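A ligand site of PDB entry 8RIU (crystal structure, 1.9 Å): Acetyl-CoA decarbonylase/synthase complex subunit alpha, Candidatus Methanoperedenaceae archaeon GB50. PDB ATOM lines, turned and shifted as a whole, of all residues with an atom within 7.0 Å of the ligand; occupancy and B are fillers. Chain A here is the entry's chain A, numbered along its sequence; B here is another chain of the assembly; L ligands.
A sulfur (S1) of the ligand sits close to the backbone NH (N) of Cys 86 (3.3 Å).
A sulfur (S1) of the ligand sits close to the backbone NH (N) of Ala 85 (3.8 Å).
The side-chain sulfur (SG) of Cys 76 is bound to an iron atom (FE3) of the ligand, at 2.3 Å.
A sulfur (S3) of the ligand lies close to the guanidinium group of Arg 96, 3.0 Å away.
FE4 of the ligand is bound by SG of Cys 86 (2.3 Å).
An iron atom (FE1) of the ligand is bound by the side-chain sulfur (SG) of Cys 68.
An iron atom (FE2) of the ligand is bound by the side-chain sulfur (SG) of Cys 71, at 2.3 Å.
A sulfur (S4) of the ligand lies close to the backbone NH of Cys 71, at 3.6 Å.
The side-chain hydroxyl of Thr 176 lies close to a sulfur (S3) of the ligand (3.3 Å).
A sulfur (S4) of the ligand lies close to the backbone NH of Phe 70, at 3.8 Å.
SG of Cys 86 sits close to N of Leu 88 (3.7 Å).
SG of Cys 68 lies close to N of Phe 70 (3.6 Å).
OG1 of Thr 176 lies within hydrogen-bond range of NE2 of Gln 621 of chain B (2.8 Å).
SG of Cys 71 sits close to SD of Met 619 of chain B (3.8 Å).
SG of Cys 68 lies close to NE2 of Gln 93 (3.5 Å).
NH2 of Arg 96 lies within hydrogen-bond range of OE1 of Gln 93.
The side-chain sulfur (SG) of Cys 76 lies close to the guanidinium group (NH1) of Arg 445 of chain B (3.2 Å).
The guanidinium group (NH1) of Arg 96 is in hydrogen-bond range of the backbone carbonyl oxygen (O) of Val 174, 2.6 Å away.
CB of Phe 73 touches S1 of the ligand (3.9 Å).
Gly 74 touches the ligand (CA to S4, 3.7 Å).
Gly 84 touches the ligand.
Hydrophobic or aromatic side chains within 4 Å of the ligand: Phe 73 and Ala 85.
Within 4 Å of the ligand: Cys 68, Phe 70, Cys 71, Phe 73, Gly 74, Cys 76, Gly 84, Ala 85, Cys 86, Arg 96 and Thr 176.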
ATOM      1  N   MET A  67      17.968  28.801 -17.268  1.00  0.00           N
ATOM      2  CA  MET A  67      17.121  29.250 -18.380  1.00  0.00           C
ATOM      3  C   MET A  67      17.619  28.673 -19.710  1.00  0.00           C
ATOM      4  O   MET A  67      18.623  27.972 -19.693  1.00  0.00           O
ATOM      5  CB  MET A  67      17.137  30.782 -18.455  1.00  0.00           C
ATOM      6  CG  MET A  67      16.679  31.480 -17.201  1.00  0.00           C
ATOM      7  SD  MET A  67      17.040  33.259 -17.240  1.00  0.00           S
ATOM      8  CE  MET A  67      18.821  33.247 -17.116  1.00  0.00           C
ATOM      9  N   CYS A  68      16.886  28.897 -20.781  1.00  0.00           N
ATOM     10  CA  CYS A  68      17.320  28.545 -22.128  1.00  0.00           C
ATOM     11  C   CYS A  68      16.981  29.703 -23.052  1.00  0.00           C
ATOM     12  O   CYS A  68      15.860  30.215 -23.008  1.00  0.00           O
ATOM     13  CB  CYS A  68      16.659  27.260 -22.625  1.00  0.00           C
ATOM     14  SG  CYS A  68      17.186  26.802 -24.302  1.00  0.00           S
ATOM     15  N   CYS A  69      17.941  30.074 -23.899  1.00  0.00           N
ATOM     16  CA  CYS A  69      17.821  31.221 -24.795  1.00  0.00           C
ATOM     17  C   CYS A  69      17.897  30.826 -26.263  1.00  0.00           C
ATOM     18  O   CYS A  69      18.090  31.693 -27.113  1.00  0.00           O
ATOM     19  CB  CYS A  69      18.955  32.216 -24.507  1.00  0.00           C
ATOM     20  SG  CYS A  69      20.587  31.463 -24.726  1.00  0.00           S
ATOM     21  N   PHE A  70      17.812  29.536 -26.580  1.00  0.00           N
ATOM     22  CA  PHE A  70      18.117  29.033 -27.957  1.00  0.00           C
ATOM     23  C   PHE A  70      17.047  29.311 -29.016  1.00  0.00           C
ATOM     24  O   PHE A  70      17.394  29.216 -30.194  1.00  0.00           O
ATOM     25  CB  PHE A  70      18.460  27.548 -27.890  1.00  0.00           C
ATOM     26  CG  PHE A  70      19.608  27.154 -27.008  1.00  0.00           C
ATOM     27  CD1 PHE A  70      20.377  28.111 -26.352  1.00  0.00           C
ATOM     28  CD2 PHE A  70      19.942  25.821 -26.849  1.00  0.00           C
ATOM     29  CE1 PHE A  70      21.438  27.732 -25.553  1.00  0.00           C
ATOM     30  CE2 PHE A  70      21.005  25.446 -26.036  1.00  0.00           C
ATOM     31  CZ  PHE A  70      21.748  26.401 -25.398  1.00  0.00           C
ATOM     32  N   CYS A  71      15.805  29.613 -28.632  1.00  0.00           N
ATOM     33  CA  CYS A  71      14.727  29.804 -29.635  1.00  0.00           C
ATOM     34  C   CYS A  71      13.841  30.983 -29.223  1.00  0.00           C
ATOM     35  O   CYS A  71      13.867  31.343 -28.047  1.00  0.00           O
ATOM     36  CB  CYS A  71      13.971  28.499 -29.878  1.00  0.00           C
ATOM     37  SG  CYS A  71      12.416  28.320 -28.972  1.00  0.00           S
ATOM     38  N   THR A  72      13.039  31.517 -30.158  1.00  0.00           N
ATOM     39  CA  THR A  72      12.216  32.731 -29.882  1.00  0.00           C
ATOM     40  C   THR A  72      11.034  32.414 -28.948  1.00  0.00           C
ATOM     41  O   THR A  72      10.452  33.383 -28.420  1.00  0.00           O
ATOM     42  CB  THR A  72      11.748  33.384 -31.188  1.00  0.00           C
ATOM     43  OG1 THR A  72      10.676  32.608 -31.730  1.00  0.00           O
ATOM     44  CG2 THR A  72      12.859  33.532 -32.199  1.00  0.00           C
ATOM     45  N   PHE A  73      10.673  31.143 -28.755  1.00  0.00           N
ATOM     46  CA  PHE A  73       9.609  30.845 -27.760  1.00  0.00           C
ATOM     47  C   PHE A  73      10.134  31.210 -26.383  1.00  0.00           C
ATOM     48  O   PHE A  73       9.324  31.455 -25.468  1.00  0.00           O
ATOM     49  CB  PHE A  73       9.237  29.360 -27.727  1.00  0.00           C
ATOM     50  CG  PHE A  73       8.374  28.858 -28.860  1.00  0.00           C
ATOM     51  CD1 PHE A  73       7.289  29.593 -29.312  1.00  0.00           C
ATOM     52  CD2 PHE A  73       8.636  27.636 -29.462  1.00  0.00           C
ATOM     53  CE1 PHE A  73       6.498  29.119 -30.337  1.00  0.00           C
ATOM     54  CE2 PHE A  73       7.850  27.170 -30.490  1.00  0.00           C
ATOM     55  CZ  PHE A  73       6.772  27.917 -30.931  1.00  0.00           C
ATOM     56  N   GLY A  74      11.458  31.222 -26.236  1.00  0.00           N
ATOM     57  CA  GLY A  74      12.075  31.580 -24.950  1.00  0.00           C
ATOM     58  C   GLY A  74      11.919  33.057 -24.662  1.00  0.00           C
ATOM     59  O   GLY A  74      11.188  33.728 -25.400  1.00  0.00           O
ATOM     60  N   LYS A  75      12.597  33.540 -23.611  1.00  0.00           N
ATOM     61  CA  LYS A  75      13.554  32.726 -22.817  1.00  0.00           C
ATOM     62  C   LYS A  75      12.787  31.871 -21.808  1.00  0.00           C
ATOM     63  O   LYS A  75      11.960  32.426 -21.074  1.00  0.00           O
ATOM     64  CB  LYS A  75      14.523  33.647 -22.066  1.00  0.00           C
ATOM     65  CG  LYS A  75      15.661  32.950 -21.343  1.00  0.00           C
ATOM     66  CD  LYS A  75      17.011  33.569 -21.620  1.00  0.00           C
ATOM     67  CE  LYS A  75      16.998  35.080 -21.530  1.00  0.00           C
ATOM     68  NZ  LYS A  75      17.082  35.547 -20.125  1.00  0.00           N
ATOM     69  N   CYS A  76      13.088  30.569 -21.764  1.00  0.00           N
ATOM     70  CA  CYS A  76      12.336  29.663 -20.868  1.00  0.00           C
ATOM     71  C   CYS A  76      13.008  29.538 -19.499  1.00  0.00           C
ATOM     72  O   CYS A  76      14.229  29.436 -19.440  1.00  0.00           O
ATOM     73  CB  CYS A  76      12.220  28.285 -21.490  1.00  0.00           C
ATOM     74  SG  CYS A  76      11.309  28.246 -23.057  1.00  0.00           S
ATOM     75  N   ASP A  77      12.207  29.624 -18.452  1.00  0.00           N
ATOM     76  CA  ASP A  77      12.680  29.320 -17.111  1.00  0.00           C
ATOM     77  C   ASP A  77      12.464  27.834 -16.861  1.00  0.00           C
ATOM     78  O   ASP A  77      11.333  27.345 -16.929  1.00  0.00           O
ATOM     79  CB  ASP A  77      11.957  30.128 -16.039  1.00  0.00           C
ATOM     80  CG  ASP A  77      12.307  29.678 -14.634  1.00  0.00           C
ATOM     81  OD1 ASP A  77      13.509  29.459 -14.378  1.00  0.00           O
ATOM     82  OD2 ASP A  77      11.396  29.539 -13.784  1.00  0.00           O
ATOM     83  N   LEU A  78      13.550  27.113 -16.576  1.00  0.00           N
ATOM     84  CA  LEU A  78      13.495  25.683 -16.295  1.00  0.00           C
ATOM     85  C   LEU A  78      13.700  25.378 -14.824  1.00  0.00           C
ATOM     86  O   LEU A  78      13.820  24.200 -14.459  1.00  0.00           O
ATOM     87  CB  LEU A  78      14.530  24.958 -17.149  1.00  0.00           C
ATOM     88  CG  LEU A  78      14.508  25.309 -18.642  1.00  0.00           C
ATOM     89  CD1 LEU A  78      15.675  24.653 -19.376  1.00  0.00           C
ATOM     90  CD2 LEU A  78      13.202  24.891 -19.284  1.00  0.00           C
ATOM     91  N   LYS A  83       9.676  22.099 -17.717  1.00  0.00           N
ATOM     92  CA  LYS A  83       9.899  21.895 -19.145  1.00  0.00           C
ATOM     93  C   LYS A  83       9.826  23.220 -19.883  1.00  0.00           C
ATOM     94  O   LYS A  83       9.012  24.088 -19.541  1.00  0.00           O
ATOM     95  CB  LYS A  83       8.865  20.926 -19.735  1.00  0.00           C
ATOM     96  CG  LYS A  83       8.841  19.550 -19.074  1.00  0.00           C
ATOM     97  CD  LYS A  83       7.895  18.576 -19.791  1.00  0.00           C
ATOM     98  CE  LYS A  83       6.473  19.108 -19.863  1.00  0.00           C
ATOM     99  NZ  LYS A  83       5.469  18.060 -20.234  1.00  0.00           N
ATOM    100  N   GLY A  84      10.662  23.359 -20.901  1.00  0.00           N
ATOM    101  CA  GLY A  84      10.625  24.549 -21.738  1.00  0.00           C
ATOM    102  C   GLY A  84       9.385  24.606 -22.610  1.00  0.00           C
ATOM    103  O   GLY A  84       8.528  23.722 -22.639  1.00  0.00           O
ATOM    104  N   ALA A  85       9.301  25.703 -23.372  1.00  0.00           N
ATOM    105  CA  ALA A  85       8.191  25.905 -24.300  1.00  0.00           C
ATOM    106  C   ALA A  85       8.161  24.879 -25.415  1.00  0.00           C
ATOM    107  O   ALA A  85       7.140  24.768 -26.105  1.00  0.00           O
ATOM    108  CB  ALA A  85       8.265  27.312 -24.887  1.00  0.00           C
ATOM    109  N   CYS A  86       9.247  24.131 -25.618  1.00  0.00           N
ATOM    110  CA  CYS A  86       9.338  23.080 -26.616  1.00  0.00           C
ATOM    111  C   CYS A  86       9.079  21.684 -26.060  1.00  0.00           C
ATOM    112  O   CYS A  86       9.106  20.712 -26.820  1.00  0.00           O
ATOM    113  CB  CYS A  86      10.719  23.102 -27.271  1.00  0.00           C
ATOM    114  SG  CYS A  86      12.062  22.906 -26.070  1.00  0.00           S
ATOM    115  N   GLY A  87       8.859  21.558 -24.740  1.00  0.00           N
ATOM    116  CA  GLY A  87       8.657  20.283 -24.092  1.00  0.00           C
ATOM    117  C   GLY A  87       9.873  19.733 -23.376  1.00  0.00           C
ATOM    118  O   GLY A  87       9.753  18.735 -22.646  1.00  0.00           O
ATOM    119  N   LEU A  88      11.046  20.313 -23.635  1.00  0.00           N
ATOM    120  CA  LEU A  88      12.313  19.764 -23.066  1.00  0.00           C
ATOM    121  C   LEU A  88      12.421  20.107 -21.578  1.00  0.00           C
ATOM    122  O   LEU A  88      12.277  21.293 -21.239  1.00  0.00           O
ATOM    123  CB  LEU A  88      13.494  20.339 -23.842  1.00  0.00           C
ATOM    124  CG  LEU A  88      14.826  19.613 -23.638  1.00  0.00           C
ATOM    125  CD1 LEU A  88      14.813  18.271 -24.349  1.00  0.00           C
ATOM    126  CD2 LEU A  88      15.987  20.467 -24.135  1.00  0.00           C
ATOM    127  N   GLN A  93      17.810  19.692 -20.955  1.00  0.00           N
ATOM    128  CA  GLN A  93      18.475  20.886 -21.462  1.00  0.00           C
ATOM    129  C   GLN A  93      19.927  20.953 -20.999  1.00  0.00           C
ATOM    130  O   GLN A  93      20.804  21.361 -21.757  1.00  0.00           O
ATOM    131  CB  GLN A  93      17.702  22.138 -21.025  1.00  0.00           C
ATOM    132  CG  GLN A  93      18.417  23.461 -21.219  1.00  0.00           C
ATOM    133  CD  GLN A  93      18.721  23.760 -22.672  1.00  0.00           C
ATOM    134  OE1 GLN A  93      18.139  23.174 -23.588  1.00  0.00           O
ATOM    135  NE2 GLN A  93      19.632  24.692 -22.893  1.00  0.00           N
ATOM    136  N   ARG A  96      21.816  18.715 -23.173  1.00  0.00           N
ATOM    137  CA  ARG A  96      21.973  19.343 -24.507  1.00  0.00           C
ATOM    138  C   ARG A  96      23.123  20.344 -24.445  1.00  0.00           C
ATOM    139  O   ARG A  96      23.914  20.382 -25.377  1.00  0.00           O
ATOM    140  CB  ARG A  96      20.688  20.058 -24.928  1.00  0.00           C
ATOM    141  CG  ARG A  96      20.812  20.832 -26.233  1.00  0.00           C
ATOM    142  CD  ARG A  96      19.507  21.008 -26.967  1.00  0.00           C
ATOM    143  NE  ARG A  96      18.670  22.021 -26.337  1.00  0.00           N
ATOM    144  CZ  ARG A  96      17.900  22.875 -26.988  1.00  0.00           C
ATOM    145  NH1 ARG A  96      17.848  22.868 -28.310  1.00  0.00           N
ATOM    146  NH2 ARG A  96      17.160  23.742 -26.307  1.00  0.00           N
ATOM    147  N   VAL A 174      20.778  18.778 -31.528  1.00  0.00           N
ATOM    148  CA  VAL A 174      20.670  19.842 -30.494  1.00  0.00           C
ATOM    149  C   VAL A 174      19.659  20.886 -30.960  1.00  0.00           C
ATOM    150  O   VAL A 174      19.382  21.825 -30.196  1.00  0.00           O
ATOM    151  CB  VAL A 174      22.046  20.435 -30.139  1.00  0.00           C
ATOM    152  CG1 VAL A 174      23.120  19.353 -30.040  1.00  0.00           C
ATOM    153  CG2 VAL A 174      22.465  21.525 -31.103  1.00  0.00           C
ATOM    154  N   HIS A 175      19.123  20.727 -32.172  1.00  0.00           N
ATOM    155  CA  HIS A 175      18.060  21.651 -32.650  1.00  0.00           C
ATOM    156  C   HIS A 175      16.802  21.472 -31.789  1.00  0.00           C
ATOM    157  O   HIS A 175      16.541  20.351 -31.310  1.00  0.00           O
ATOM    158  CB  HIS A 175      17.747  21.434 -34.132  1.00  0.00           C
ATOM    159  CG  HIS A 175      16.855  22.483 -34.711  1.00  0.00           C
ATOM    160  ND1 HIS A 175      15.501  22.536 -34.458  1.00  0.00           N
ATOM    161  CD2 HIS A 175      17.117  23.525 -35.508  1.00  0.00           C
ATOM    162  CE1 HIS A 175      14.981  23.570 -35.087  1.00  0.00           C
ATOM    163  NE2 HIS A 175      15.940  24.189 -35.737  1.00  0.00           N
ATOM    164  N   THR A 176      16.065  22.550 -31.590  1.00  0.00           N
ATOM    165  CA  THR A 176      14.825  22.508 -30.836  1.00  0.00           C
ATOM    166  C   THR A 176      13.914  21.419 -31.393  1.00  0.00           C
ATOM    167  O   THR A 176      13.815  21.217 -32.611  1.00  0.00           O
ATOM    168  CB  THR A 176      14.106  23.854 -30.906  1.00  0.00           C
ATOM    169  OG1 THR A 176      14.990  24.903 -30.475  1.00  0.00           O
ATOM    170  CG2 THR A 176      12.865  23.831 -30.032  1.00  0.00           C
ATOM    171  N   GLY A 177      13.248  20.712 -30.482  1.00  0.00           N
ATOM    172  CA  GLY A 177      12.332  19.666 -30.895  1.00  0.00           C
ATOM    173  C   GLY A 177      13.024  18.404 -31.370  1.00  0.00           C
ATOM    174  O   GLY A 177      12.605  17.816 -32.373  1.00  0.00           O
ATOM    175  N   CYS B 443       2.685  25.752 -26.110  1.00  0.00           N
ATOM    176  CA  CYS B 443       3.999  25.554 -25.490  1.00  0.00           C
ATOM    177  C   CYS B 443       3.933  24.902 -24.123  1.00  0.00           C
ATOM    178  O   CYS B 443       4.918  24.268 -23.716  1.00  0.00           O
ATOM    179  CB  CYS B 443       4.745  26.888 -25.357  1.00  0.00           C
ATOM    180  SG  CYS B 443       4.100  27.966 -24.060  1.00  0.00           S
ATOM    181  N   ARG B 445       3.863  26.284 -21.076  1.00  0.00           N
ATOM    182  CA  ARG B 445       4.544  26.897 -19.935  1.00  0.00           C
ATOM    183  C   ARG B 445       3.558  27.376 -18.872  1.00  0.00           C
ATOM    184  O   ARG B 445       3.867  27.340 -17.680  1.00  0.00           O
ATOM    185  CB  ARG B 445       5.424  28.062 -20.402  1.00  0.00           C
ATOM    186  CG  ARG B 445       6.667  27.624 -21.192  1.00  0.00           C
ATOM    187  CD  ARG B 445       7.854  28.572 -21.038  1.00  0.00           C
ATOM    188  NE  ARG B 445       7.481  29.975 -21.212  1.00  0.00           N
ATOM    189  CZ  ARG B 445       7.995  30.799 -22.113  1.00  0.00           C
ATOM    190  NH1 ARG B 445       8.901  30.380 -22.984  1.00  0.00           N
ATOM    191  NH2 ARG B 445       7.578  32.052 -22.159  1.00  0.00           N
ATOM    192  N   MET B 619      11.229  31.170 -35.186  1.00  0.00           N
ATOM    193  CA  MET B 619      11.474  30.643 -33.842  1.00  0.00           C
ATOM    194  C   MET B 619      12.744  29.808 -33.808  1.00  0.00           C
ATOM    195  O   MET B 619      13.601  30.006 -32.936  1.00  0.00           O
ATOM    196  CB  MET B 619      10.242  29.832 -33.393  1.00  0.00           C
ATOM    197  CG  MET B 619      10.402  28.890 -32.167  1.00  0.00           C
ATOM    198  SD  MET B 619      11.306  27.346 -32.442  1.00  0.00           S
ATOM    199  CE  MET B 619      10.201  26.556 -33.635  1.00  0.00           C
ATOM    200  N   GLN B 621      16.271  27.421 -34.839  1.00  0.00           N
ATOM    201  CA  GLN B 621      17.632  27.660 -35.315  1.00  0.00           C
ATOM    202  C   GLN B 621      17.721  27.516 -36.825  1.00  0.00           C
ATOM    203  O   GLN B 621      18.453  28.254 -37.493  1.00  0.00           O
ATOM    204  CB  GLN B 621      18.610  26.701 -34.639  1.00  0.00           C
ATOM    205  CG  GLN B 621      18.703  26.839 -33.122  1.00  0.00           C
ATOM    206  CD  GLN B 621      17.652  26.030 -32.407  1.00  0.00           C
ATOM    207  OE1 GLN B 621      17.253  24.959 -32.871  1.00  0.00           O
ATOM    208  NE2 GLN B 621      17.174  26.543 -31.284  1.00  0.00           N
HETATM  209 FE1  LIG L   1      15.119  26.565 -25.253  1.00  0.00          FE
HETATM  210 FE2  LIG L   1      13.434  27.280 -27.169  1.00  0.00          FE
HETATM  211 FE3  LIG L   1      12.724  27.256 -24.602  1.00  0.00          FE
HETATM  212 FE4  LIG L   1      13.080  24.929 -25.825  1.00  0.00          FE
HETATM  213  S1  LIG L   1      11.473  26.483 -26.328  1.00  0.00           S
HETATM  214  S2  LIG L   1      13.791  25.460 -23.719  1.00  0.00           S
HETATM  215  S3  LIG L   1      14.847  25.484 -27.239  1.00  0.00           S
HETATM  216  S4  LIG L   1      14.282  28.673 -25.550  1.00  0.00           S
